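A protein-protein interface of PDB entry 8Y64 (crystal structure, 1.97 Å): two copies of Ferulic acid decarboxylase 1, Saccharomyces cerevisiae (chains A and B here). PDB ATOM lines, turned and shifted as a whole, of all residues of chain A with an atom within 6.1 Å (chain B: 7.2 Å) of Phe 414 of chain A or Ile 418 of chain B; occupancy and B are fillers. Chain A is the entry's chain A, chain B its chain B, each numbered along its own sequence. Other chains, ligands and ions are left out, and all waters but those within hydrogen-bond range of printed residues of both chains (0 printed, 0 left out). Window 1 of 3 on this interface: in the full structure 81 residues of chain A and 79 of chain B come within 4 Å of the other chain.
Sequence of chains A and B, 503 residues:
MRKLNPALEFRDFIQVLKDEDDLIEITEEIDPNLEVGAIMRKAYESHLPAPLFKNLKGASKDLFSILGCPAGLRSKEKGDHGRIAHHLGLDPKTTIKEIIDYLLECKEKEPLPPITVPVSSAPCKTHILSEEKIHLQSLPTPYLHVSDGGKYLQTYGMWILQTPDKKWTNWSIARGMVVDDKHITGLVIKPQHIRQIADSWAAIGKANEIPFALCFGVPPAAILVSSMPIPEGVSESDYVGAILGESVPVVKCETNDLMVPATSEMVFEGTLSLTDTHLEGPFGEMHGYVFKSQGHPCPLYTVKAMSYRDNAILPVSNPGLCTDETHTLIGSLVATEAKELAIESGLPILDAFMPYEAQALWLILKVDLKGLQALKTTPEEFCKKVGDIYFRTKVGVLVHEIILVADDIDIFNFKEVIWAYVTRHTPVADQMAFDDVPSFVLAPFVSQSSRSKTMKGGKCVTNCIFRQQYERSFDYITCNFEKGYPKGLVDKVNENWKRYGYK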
ATOM      1  N   PRO A 355       9.208   8.294  21.199  1.00  0.00           N
ATOM      2  CA  PRO A 355       8.520   8.934  22.334  1.00  0.00           C
ATOM      3  C   PRO A 355       8.248   7.968  23.473  1.00  0.00           C
ATOM      4  O   PRO A 355       7.783   6.844  23.266  1.00  0.00           O
ATOM      5  CB  PRO A 355       7.212   9.446  21.720  1.00  0.00           C
ATOM      6  CG  PRO A 355       7.554   9.653  20.244  1.00  0.00           C
ATOM      7  CD  PRO A 355       8.490   8.500  19.924  1.00  0.00           C
ATOM      8  N   TYR A 356       8.509   8.449  24.692  1.00  0.00           N
ATOM      9  CA  TYR A 356       8.353   7.618  25.884  1.00  0.00           C
ATOM     10  C   TYR A 356       6.901   7.190  26.069  1.00  0.00           C
ATOM     11  O   TYR A 356       6.629   6.044  26.448  1.00  0.00           O
ATOM     12  CB  TYR A 356       8.856   8.376  27.115  1.00  0.00           C
ATOM     13  CG  TYR A 356      10.250   8.973  26.953  1.00  0.00           C
ATOM     14  CD1 TYR A 356      11.223   8.325  26.201  1.00  0.00           C
ATOM     15  CD2 TYR A 356      10.585  10.181  27.554  1.00  0.00           C
ATOM     16  CE1 TYR A 356      12.484   8.870  26.034  1.00  0.00           C
ATOM     17  CE2 TYR A 356      11.856  10.732  27.404  1.00  0.00           C
ATOM     18  CZ  TYR A 356      12.794  10.072  26.640  1.00  0.00           C
ATOM     19  OH  TYR A 356      14.058  10.608  26.479  1.00  0.00           O
ATOM     20  N   GLU A 357       5.956   8.092  25.772  1.00  0.00           N
ATOM     21  CA  GLU A 357       4.528   7.791  25.909  1.00  0.00           C
ATOM     22  C   GLU A 357       4.084   6.629  25.020  1.00  0.00           C
ATOM     23  O   GLU A 357       3.057   6.005  25.302  1.00  0.00           O
ATOM     24  CB  GLU A 357       3.710   9.055  25.590  1.00  0.00           C
ATOM     25  CG  GLU A 357       3.901  10.188  26.608  1.00  0.00           C
ATOM     26  CD  GLU A 357       5.065  11.155  26.261  1.00  0.00           C
ATOM     27  OE1 GLU A 357       5.963  10.812  25.446  1.00  0.00           O
ATOM     28  OE2 GLU A 357       5.115  12.241  26.867  1.00  0.00           O
ATOM     29  N   ALA A 358       4.820   6.323  23.949  1.00  0.00           N
ATOM     30  CA  ALA A 358       4.505   5.178  23.108  1.00  0.00           C
ATOM     31  C   ALA A 358       5.323   3.943  23.478  1.00  0.00           C
ATOM     32  O   ALA A 358       5.414   3.011  22.682  1.00  0.00           O
ATOM     33  CB  ALA A 358       4.694   5.537  21.627  1.00  0.00           C
ATOM     34  N   TRP A 362       7.084   3.445  18.918  1.00  0.00           N
ATOM     35  CA  TRP A 362       6.983   4.422  17.845  1.00  0.00           C
ATOM     36  C   TRP A 362       8.342   5.055  17.593  1.00  0.00           C
ATOM     37  O   TRP A 362       8.962   5.562  18.525  1.00  0.00           O
ATOM     38  CB  TRP A 362       6.008   5.539  18.218  1.00  0.00           C
ATOM     39  CG  TRP A 362       4.543   5.224  18.123  1.00  0.00           C
ATOM     40  CD1 TRP A 362       3.969   4.018  17.903  1.00  0.00           C
ATOM     41  CD2 TRP A 362       3.477   6.179  18.199  1.00  0.00           C
ATOM     42  NE1 TRP A 362       2.589   4.153  17.864  1.00  0.00           N
ATOM     43  CE2 TRP A 362       2.271   5.473  18.039  1.00  0.00           C
ATOM     44  CE3 TRP A 362       3.431   7.570  18.408  1.00  0.00           C
ATOM     45  CZ2 TRP A 362       1.028   6.101  18.070  1.00  0.00           C
ATOM     46  CZ3 TRP A 362       2.203   8.190  18.443  1.00  0.00           C
ATOM     47  CH2 TRP A 362       1.015   7.459  18.264  1.00  0.00           C
ATOM     48  N   ASP A 410       8.273  19.520  16.565  1.00  0.00           N
ATOM     49  CA  ASP A 410       9.304  19.179  17.551  1.00  0.00           C
ATOM     50  C   ASP A 410       9.042  17.754  18.031  1.00  0.00           C
ATOM     51  O   ASP A 410       8.191  17.512  18.897  1.00  0.00           O
ATOM     52  CB  ASP A 410       9.305  20.180  18.702  1.00  0.00           C
ATOM     53  CG  ASP A 410      10.363  19.868  19.753  1.00  0.00           C
ATOM     54  OD1 ASP A 410      11.199  18.972  19.521  1.00  0.00           O
ATOM     55  OD2 ASP A 410      10.366  20.529  20.812  1.00  0.00           O
ATOM     56  N   ILE A 411       9.785  16.796  17.477  1.00  0.00           N
ATOM     57  CA  ILE A 411       9.483  15.395  17.730  1.00  0.00           C
ATOM     58  C   ILE A 411       9.837  14.984  19.145  1.00  0.00           C
ATOM     59  O   ILE A 411       9.437  13.900  19.584  1.00  0.00           O
ATOM     60  CB  ILE A 411      10.196  14.474  16.712  1.00  0.00           C
ATOM     61  CG1 ILE A 411      11.716  14.521  16.878  1.00  0.00           C
ATOM     62  CG2 ILE A 411       9.783  14.803  15.267  1.00  0.00           C
ATOM     63  CD1 ILE A 411      12.448  13.422  16.033  1.00  0.00           C
ATOM     64  N   PHE A 412      10.587  15.815  19.867  1.00  0.00           N
ATOM     65  CA  PHE A 412      10.922  15.545  21.259  1.00  0.00           C
ATOM     66  C   PHE A 412       9.833  16.016  22.209  1.00  0.00           C
ATOM     67  O   PHE A 412       9.940  15.805  23.418  1.00  0.00           O
ATOM     68  CB  PHE A 412      12.265  16.203  21.591  1.00  0.00           C
ATOM     69  CG  PHE A 412      13.378  15.716  20.708  1.00  0.00           C
ATOM     70  CD1 PHE A 412      13.882  14.439  20.868  1.00  0.00           C
ATOM     71  CD2 PHE A 412      13.862  16.500  19.675  1.00  0.00           C
ATOM     72  CE1 PHE A 412      14.883  13.961  20.029  1.00  0.00           C
ATOM     73  CE2 PHE A 412      14.859  16.028  18.833  1.00  0.00           C
ATOM     74  CZ  PHE A 412      15.374  14.759  19.022  1.00  0.00           C
ATOM     75  N   ASN A 413       8.776  16.616  21.679  1.00  0.00           N
ATOM     76  CA  ASN A 413       7.664  17.156  22.456  1.00  0.00           C
ATOM     77  C   ASN A 413       6.415  16.369  22.087  1.00  0.00           C
ATOM     78  O   ASN A 413       5.826  16.609  21.031  1.00  0.00           O
ATOM     79  CB  ASN A 413       7.481  18.646  22.161  1.00  0.00           C
ATOM     80  CG  ASN A 413       6.408  19.269  23.007  1.00  0.00           C
ATOM     81  OD1 ASN A 413       5.646  18.562  23.664  1.00  0.00           O
ATOM     82  ND2 ASN A 413       6.349  20.600  23.013  1.00  0.00           N
ATOM     83  N   PHE A 414       5.970  15.468  22.966  1.00  0.00           N
ATOM     84  CA  PHE A 414       4.872  14.593  22.575  1.00  0.00           C
ATOM     85  C   PHE A 414       3.577  15.359  22.316  1.00  0.00           C
ATOM     86  O   PHE A 414       2.706  14.846  21.606  1.00  0.00           O
ATOM     87  CB  PHE A 414       4.651  13.509  23.632  1.00  0.00           C
ATOM     88  CG  PHE A 414       3.792  12.385  23.151  1.00  0.00           C
ATOM     89  CD1 PHE A 414       4.181  11.619  22.066  1.00  0.00           C
ATOM     90  CD2 PHE A 414       2.580  12.111  23.762  1.00  0.00           C
ATOM     91  CE1 PHE A 414       3.397  10.582  21.605  1.00  0.00           C
ATOM     92  CE2 PHE A 414       1.782  11.063  23.304  1.00  0.00           C
ATOM     93  CZ  PHE A 414       2.195  10.300  22.222  1.00  0.00           C
ATOM     94  N   LYS A 415       3.445  16.581  22.843  1.00  0.00           N
ATOM     95  CA  LYS A 415       2.276  17.398  22.519  1.00  0.00           C
ATOM     96  C   LYS A 415       2.213  17.665  21.031  1.00  0.00           C
ATOM     97  O   LYS A 415       1.140  17.588  20.428  1.00  0.00           O
ATOM     98  CB  LYS A 415       2.315  18.724  23.278  1.00  0.00           C
ATOM     99  CG  LYS A 415       2.018  18.608  24.774  1.00  0.00           C
ATOM    100  CD  LYS A 415       1.971  20.008  25.391  1.00  0.00           C
ATOM    101  CE  LYS A 415       1.451  19.979  26.824  1.00  0.00           C
ATOM    102  NZ  LYS A 415       1.898  21.204  27.558  1.00  0.00           N
ATOM    103  N   GLU A 416       3.363  17.963  20.417  1.00  0.00           N
ATOM    104  CA  GLU A 416       3.392  18.207  18.978  1.00  0.00           C
ATOM    105  C   GLU A 416       3.272  16.916  18.188  1.00  0.00           C
ATOM    106  O   GLU A 416       2.627  16.914  17.137  1.00  0.00           O
ATOM    107  CB  GLU A 416       4.674  18.949  18.601  1.00  0.00           C
ATOM    108  CG  GLU A 416       4.777  20.292  19.321  1.00  0.00           C
ATOM    109  CD  GLU A 416       5.792  21.247  18.712  1.00  0.00           C
ATOM    110  OE1 GLU A 416       6.186  21.074  17.530  1.00  0.00           O
ATOM    111  OE2 GLU A 416       6.207  22.168  19.445  1.00  0.00           O
ATOM    112  N   VAL A 417       3.839  15.809  18.697  1.00  0.00           N
ATOM    113  CA  VAL A 417       3.808  14.547  17.960  1.00  0.00           C
ATOM    114  C   VAL A 417       2.385  14.005  17.855  1.00  0.00           C
ATOM    115  O   VAL A 417       1.960  13.563  16.776  1.00  0.00           O
ATOM    116  CB  VAL A 417       4.743  13.508  18.610  1.00  0.00           C
ATOM    117  CG1 VAL A 417       4.523  12.148  17.977  1.00  0.00           C
ATOM    118  CG2 VAL A 417       6.212  13.944  18.462  1.00  0.00           C
ATOM    119  N   ILE A 418       1.657  13.951  18.979  1.00  0.00           N
ATOM    120  CA  ILE A 418       0.306  13.377  18.950  1.00  0.00           C
ATOM    121  C   ILE A 418      -0.615  14.238  18.087  1.00  0.00           C
ATOM    122  O   ILE A 418      -1.464  13.720  17.344  1.00  0.00           O
ATOM    123  CB  ILE A 418      -0.237  13.173  20.386  1.00  0.00           C
ATOM    124  CG1 ILE A 418      -1.482  12.270  20.394  1.00  0.00           C
ATOM    125  CG2 ILE A 418      -0.587  14.489  21.083  1.00  0.00           C
ATOM    126  CD1 ILE A 418      -1.270  10.917  19.754  1.00  0.00           C
ATOM    127  N   TRP A 419      -0.412  15.554  18.116  1.00  0.00           N
ATOM    128  CA  TRP A 419      -1.173  16.457  17.253  1.00  0.00           C
ATOM    129  C   TRP A 419      -0.921  16.156  15.784  1.00  0.00           C
ATOM    130  O   TRP A 419      -1.860  16.028  14.986  1.00  0.00           O
ATOM    131  CB  TRP A 419      -0.787  17.897  17.555  1.00  0.00           C
ATOM    132  CG  TRP A 419      -1.387  18.917  16.588  1.00  0.00           C
ATOM    133  CD1 TRP A 419      -2.724  19.152  16.347  1.00  0.00           C
ATOM    134  CD2 TRP A 419      -0.665  19.856  15.783  1.00  0.00           C
ATOM    135  NE1 TRP A 419      -2.869  20.175  15.428  1.00  0.00           N
ATOM    136  CE2 TRP A 419      -1.621  20.629  15.076  1.00  0.00           C
ATOM    137  CE3 TRP A 419       0.699  20.120  15.591  1.00  0.00           C
ATOM    138  CZ2 TRP A 419      -1.248  21.649  14.193  1.00  0.00           C
ATOM    139  CZ3 TRP A 419       1.066  21.136  14.703  1.00  0.00           C
ATOM    140  CH2 TRP A 419       0.097  21.880  14.016  1.00  0.00           C
ATOM    141  N   GLU B 357      -6.489  15.359  23.498  1.00  0.00           N
ATOM    142  CA  GLU B 357      -5.195  15.317  22.818  1.00  0.00           C
ATOM    143  C   GLU B 357      -5.322  14.814  21.389  1.00  0.00           C
ATOM    144  O   GLU B 357      -4.423  15.044  20.568  1.00  0.00           O
ATOM    145  CB  GLU B 357      -4.229  14.430  23.616  1.00  0.00           C
ATOM    146  CG  GLU B 357      -3.852  15.027  24.994  1.00  0.00           C
ATOM    147  CD  GLU B 357      -4.793  14.620  26.136  1.00  0.00           C
ATOM    148  OE1 GLU B 357      -5.927  14.160  25.890  1.00  0.00           O
ATOM    149  OE2 GLU B 357      -4.399  14.793  27.307  1.00  0.00           O
ATOM    150  N   TRP B 362     -10.670  11.092  17.700  1.00  0.00           N
ATOM    151  CA  TRP B 362     -10.705   9.732  18.232  1.00  0.00           C
ATOM    152  C   TRP B 362     -11.903   9.582  19.169  1.00  0.00           C
ATOM    153  O   TRP B 362     -12.086  10.401  20.072  1.00  0.00           O
ATOM    154  CB  TRP B 362      -9.439   9.472  19.047  1.00  0.00           C
ATOM    155  CG  TRP B 362      -8.190   9.167  18.294  1.00  0.00           C
ATOM    156  CD1 TRP B 362      -7.947   9.315  16.948  1.00  0.00           C
ATOM    157  CD2 TRP B 362      -6.973   8.709  18.883  1.00  0.00           C
ATOM    158  NE1 TRP B 362      -6.633   8.927  16.668  1.00  0.00           N
ATOM    159  CE2 TRP B 362      -6.023   8.564  17.843  1.00  0.00           C
ATOM    160  CE3 TRP B 362      -6.596   8.397  20.201  1.00  0.00           C
ATOM    161  CZ2 TRP B 362      -4.724   8.101  18.080  1.00  0.00           C
ATOM    162  CZ3 TRP B 362      -5.302   7.941  20.433  1.00  0.00           C
ATOM    163  CH2 TRP B 362      -4.389   7.797  19.382  1.00  0.00           C
ATOM    164  N   ILE B 364     -12.977   6.879  21.968  1.00  0.00           N
ATOM    165  CA  ILE B 364     -12.646   5.661  22.720  1.00  0.00           C
ATOM    166  C   ILE B 364     -13.920   5.077  23.302  1.00  0.00           C
ATOM    167  O   ILE B 364     -14.693   5.790  23.957  1.00  0.00           O
ATOM    168  CB  ILE B 364     -11.643   5.928  23.855  1.00  0.00           C
ATOM    169  CG1 ILE B 364     -10.612   6.978  23.453  1.00  0.00           C
ATOM    170  CG2 ILE B 364     -10.998   4.592  24.325  1.00  0.00           C
ATOM    171  CD1 ILE B 364      -9.641   6.492  22.392  1.00  0.00           C
ATOM    172  N   ILE B 409      -9.172   0.173  31.418  1.00  0.00           N
ATOM    173  CA  ILE B 409      -8.625   1.447  30.957  1.00  0.00           C
ATOM    174  C   ILE B 409      -9.563   2.572  31.375  1.00  0.00           C
ATOM    175  O   ILE B 409     -10.748   2.566  31.011  1.00  0.00           O
ATOM    176  CB  ILE B 409      -8.426   1.451  29.432  1.00  0.00           C
ATOM    177  CG1 ILE B 409      -7.398   0.405  29.026  1.00  0.00           C
ATOM    178  CG2 ILE B 409      -8.006   2.853  28.936  1.00  0.00           C
ATOM    179  CD1 ILE B 409      -6.059   0.550  29.751  1.00  0.00           C
ATOM    180  N   ASN B 413      -8.503   9.374  31.007  1.00  0.00           N
ATOM    181  CA  ASN B 413      -7.121   9.725  31.330  1.00  0.00           C
ATOM    182  C   ASN B 413      -6.279   9.370  30.114  1.00  0.00           C
ATOM    183  O   ASN B 413      -6.124   8.191  29.790  1.00  0.00           O
ATOM    184  CB  ASN B 413      -6.673   8.975  32.591  1.00  0.00           C
ATOM    185  CG  ASN B 413      -5.224   9.267  32.991  1.00  0.00           C
ATOM    186  OD1 ASN B 413      -4.485   9.961  32.288  1.00  0.00           O
ATOM    187  ND2 ASN B 413      -4.834   8.765  34.162  1.00  0.00           N
ATOM    188  N   PHE B 414      -5.745  10.382  29.423  1.00  0.00           N
ATOM    189  CA  PHE B 414      -5.047  10.070  28.186  1.00  0.00           C
ATOM    190  C   PHE B 414      -3.764   9.280  28.429  1.00  0.00           C
ATOM    191  O   PHE B 414      -3.281   8.626  27.505  1.00  0.00           O
ATOM    192  CB  PHE B 414      -4.763  11.345  27.393  1.00  0.00           C
ATOM    193  CG  PHE B 414      -4.338  11.081  25.973  1.00  0.00           C
ATOM    194  CD1 PHE B 414      -5.183  10.426  25.090  1.00  0.00           C
ATOM    195  CD2 PHE B 414      -3.077  11.455  25.538  1.00  0.00           C
ATOM    196  CE1 PHE B 414      -4.782  10.170  23.764  1.00  0.00           C
ATOM    197  CE2 PHE B 414      -2.674  11.218  24.233  1.00  0.00           C
ATOM    198  CZ  PHE B 414      -3.523  10.567  23.350  1.00  0.00           C
ATOM    199  N   LYS B 415      -3.225   9.287  29.656  1.00  0.00           N
ATOM    200  CA  LYS B 415      -2.059   8.453  29.946  1.00  0.00           C
ATOM    201  C   LYS B 415      -2.389   6.976  29.762  1.00  0.00           C
ATOM    202  O   LYS B 415      -1.584   6.214  29.215  1.00  0.00           O
ATOM    203  CB  LYS B 415      -1.549   8.704  31.373  1.00  0.00           C
ATOM    204  CG  LYS B 415      -0.905  10.063  31.590  1.00  0.00           C
ATOM    205  CD  LYS B 415      -0.374  10.225  33.017  1.00  0.00           C
ATOM    206  CE  LYS B 415       0.820  11.187  33.038  1.00  0.00           C
ATOM    207  NZ  LYS B 415       0.990  11.879  34.348  1.00  0.00           N
ATOM    208  N   GLU B 416      -3.564   6.552  30.216  1.00  0.00           N
ATOM    209  CA  GLU B 416      -3.986   5.169  30.028  1.00  0.00           C
ATOM    210  C   GLU B 416      -4.421   4.906  28.592  1.00  0.00           C
ATOM    211  O   GLU B 416      -4.152   3.828  28.053  1.00  0.00           O
ATOM    212  CB  GLU B 416      -5.111   4.838  31.017  1.00  0.00           C
ATOM    213  CG  GLU B 416      -4.663   5.057  32.456  1.00  0.00           C
ATOM    214  CD  GLU B 416      -5.531   4.372  33.491  1.00  0.00           C
ATOM    215  OE1 GLU B 416      -6.364   3.495  33.129  1.00  0.00           O
ATOM    216  OE2 GLU B 416      -5.371   4.739  34.676  1.00  0.00           O
ATOM    217  N   VAL B 417      -5.026   5.897  27.938  1.00  0.00           N
ATOM    218  CA  VAL B 417      -5.487   5.714  26.563  1.00  0.00           C
ATOM    219  C   VAL B 417      -4.318   5.495  25.602  1.00  0.00           C
ATOM    220  O   VAL B 417      -4.357   4.584  24.767  1.00  0.00           O
ATOM    221  CB  VAL B 417      -6.353   6.907  26.121  1.00  0.00           C
ATOM    222  CG1 VAL B 417      -6.627   6.806  24.625  1.00  0.00           C
ATOM    223  CG2 VAL B 417      -7.677   6.902  26.904  1.00  0.00           C
ATOM    224  N   ILE B 418      -3.290   6.355  25.653  1.00  0.00           N
ATOM    225  CA  ILE B 418      -2.179   6.203  24.705  1.00  0.00           C
ATOM    226  C   ILE B 418      -1.418   4.917  24.996  1.00  0.00           C
ATOM    227  O   ILE B 418      -0.967   4.225  24.073  1.00  0.00           O
ATOM    228  CB  ILE B 418      -1.243   7.439  24.713  1.00  0.00           C
ATOM    229  CG1 ILE B 418      -0.279   7.436  23.508  1.00  0.00           C
ATOM    230  CG2 ILE B 418      -0.454   7.580  26.028  1.00  0.00           C
ATOM    231  CD1 ILE B 418      -0.963   7.287  22.117  1.00  0.00           C
ATOM    232  N   TRP B 419      -1.300   4.556  26.277  1.00  0.00           N
ATOM    233  CA  TRP B 419      -0.692   3.278  26.634  1.00  0.00           C
ATOM    234  C   TRP B 419      -1.432   2.116  25.976  1.00  0.00           C
ATOM    235  O   TRP B 419      -0.825   1.265  25.308  1.00  0.00           O
ATOM    236  CB  TRP B 419      -0.688   3.112  28.162  1.00  0.00           C
ATOM    237  CG  TRP B 419      -0.177   1.770  28.606  1.00  0.00           C
ATOM    238  CD1 TRP B 419       1.056   1.226  28.330  1.00  0.00           C
ATOM    239  CD2 TRP B 419      -0.847   0.830  29.449  1.00  0.00           C
ATOM    240  NE1 TRP B 419       1.174  -0.010  28.930  1.00  0.00           N
ATOM    241  CE2 TRP B 419       0.023  -0.269  29.631  1.00  0.00           C
ATOM    242  CE3 TRP B 419      -2.101   0.806  30.066  1.00  0.00           C
ATOM    243  CZ2 TRP B 419      -0.322  -1.367  30.411  1.00  0.00           C
ATOM    244  CZ3 TRP B 419      -2.439  -0.292  30.845  1.00  0.00           C
ATOM    245  CH2 TRP B 419      -1.556  -1.369  30.994  1.00  0.00           C
ATOM    246  N   ALA B 420      -2.752   2.048  26.180  1.00  0.00           N
ATOM    247  CA  ALA B 420      -3.530   0.964  25.590  1.00  0.00           C
ATOM    248  C   ALA B 420      -3.474   1.006  24.068  1.00  0.00           C
ATOM    249  O   ALA B 420      -3.372  -0.038  23.419  1.00  0.00           O
ATOM    250  CB  ALA B 420      -4.981   1.033  26.070  1.00  0.00           C
ATOM    251  N   TYR B 421      -3.554   2.205  23.482  1.00  0.00           N
ATOM    252  CA  TYR B 421      -3.539   2.317  22.023  1.00  0.00           C
ATOM    253  C   TYR B 421      -2.269   1.712  21.434  1.00  0.00           C
ATOM    254  O   TYR B 421      -2.331   0.869  20.528  1.00  0.00           O
ATOM    255  CB  TYR B 421      -3.663   3.782  21.592  1.00  0.00           C
ATOM    256  CG  TYR B 421      -3.783   3.956  20.076  1.00  0.00           C
ATOM    257  CD1 TYR B 421      -4.990   3.684  19.426  1.00  0.00           C
ATOM    258  CD2 TYR B 421      -2.701   4.395  19.305  1.00  0.00           C
ATOM    259  CE1 TYR B 421      -5.127   3.845  18.054  1.00  0.00           C
ATOM    260  CE2 TYR B 421      -2.831   4.564  17.900  1.00  0.00           C
ATOM    261  CZ  TYR B 421      -4.051   4.282  17.296  1.00  0.00           C
ATOM    262  OH  TYR B 421      -4.227   4.422  15.930  1.00  0.00           O
ATOM    263  N   VAL B 422      -1.102   2.121  21.942  1.00  0.00           N
ATOM    264  CA  VAL B 422       0.133   1.668  21.295  1.00  0.00           C
ATOM    265  C   VAL B 422       0.447   0.207  21.629  1.00  0.00           C
ATOM    266  O   VAL B 422       1.060  -0.498  20.810  1.00  0.00           O
ATOM    267  CB  VAL B 422       1.331   2.573  21.649  1.00  0.00           C
ATOM    268  CG1 VAL B 422       1.036   4.050  21.246  1.00  0.00           C
ATOM    269  CG2 VAL B 422       1.754   2.435  23.119  1.00  0.00           C
ATOM    270  N   THR B 423       0.068  -0.277  22.810  1.00  0.00           N
ATOM    271  CA  THR B 423       0.478  -1.625  23.203  1.00  0.00           C
ATOM    272  C   THR B 423      -0.522  -2.712  22.862  1.00  0.00           C
ATOM    273  O   THR B 423      -0.142  -3.887  22.902  1.00  0.00           O
ATOM    274  CB  THR B 423       0.777  -1.710  24.711  1.00  0.00           C
ATOM    275  OG1 THR B 423      -0.408  -1.441  25.476  1.00  0.00           O
ATOM    276  CG2 THR B 423       1.887  -0.726  25.091  1.00  0.00           C
ATOM    277  N   ARG B 424      -1.776  -2.381  22.531  1.00  0.00           N
ATOM    278  CA  ARG B 424      -2.791  -3.421  22.390  1.00  0.00           C
ATOM    279  C   ARG B 424      -3.366  -3.586  20.987  1.00  0.00           C
ATOM    280  O   ARG B 424      -4.222  -4.453  20.796  1.00  0.00           O
ATOM    281  CB  ARG B 424      -3.945  -3.194  23.384  1.00  0.00           C
ATOM    282  CG  ARG B 424      -3.482  -3.084  24.844  1.00  0.00           C
ATOM    283  CD  ARG B 424      -4.649  -3.177  25.853  1.00  0.00           C
ATOM    284  NE  ARG B 424      -4.172  -2.890  27.202  1.00  0.00           N
ATOM    285  CZ  ARG B 424      -4.932  -2.872  28.291  1.00  0.00           C
ATOM    286  NH1 ARG B 424      -6.243  -3.053  28.222  1.00  0.00           N
ATOM    287  NH2 ARG B 424      -4.362  -2.650  29.482  1.00  0.00           N
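Ile 418 of chain B touches Glu 357 of chain A (CG2 to O, 3.9 Å).
CG2 of Val 422 of chain B touches O of Ala 358 of chain A, 3.7 Å away.
Val 422 of chain B touches Trp 362 of chain A (CG1 to CE2, 3.7 Å).
Phe 414 of chain A touches Ile 418 of chain B.
Glu 357 of chain B touches Ile 418 of chain A.
Phe 414 of chain B touches Ile 418 of chain A.
Of the printed residues of chain B, Phe 414 of chain A touches Ile 418 (3.997 Å).
Printed residues of chain B within 4 Å of Trp 362 of chain A: Val 422.
Of the printed residues of chain B, Glu 357 of chain A touches Ile 418 (3.9 Å).
Of the printed residues of chain A, Val 422 of chain B touches Ala 358 and Trp 362.
The nearest printed residue of chain B that does not touch Phe 414 of chain A is Phe 414 of chain B (4.6 Å).
The nearest printed residue of chain A that does not touch Ile 418 of chain B is Trp 362 of chain A (4.3 Å).
Glu 357 of chain A touches Ile 418 of chain B, and with the chains exchanged Ile 418 of chain A touches Glu 357 of chain B.
Phe 414 of chain A touches Ile 418 of chain B, and with the chains exchanged Ile 418 of chain A touches Phe 414 of chain B.
Of the 6 pairs that touch across the chains among the printed residues, 4 have their exchanged pair printed and touching as well.
Hydrophobic or aromatic side chains of chain B that line the printed part of chain A: Phe 414, Ile 418 and Val 422.
Among the printed residues, 6 pairs touch across the chains.
Among the printed residues, no Asp or Glu carboxylate lies within 4 Å of a Lys or Arg side-chain nitrogen of the other chain.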
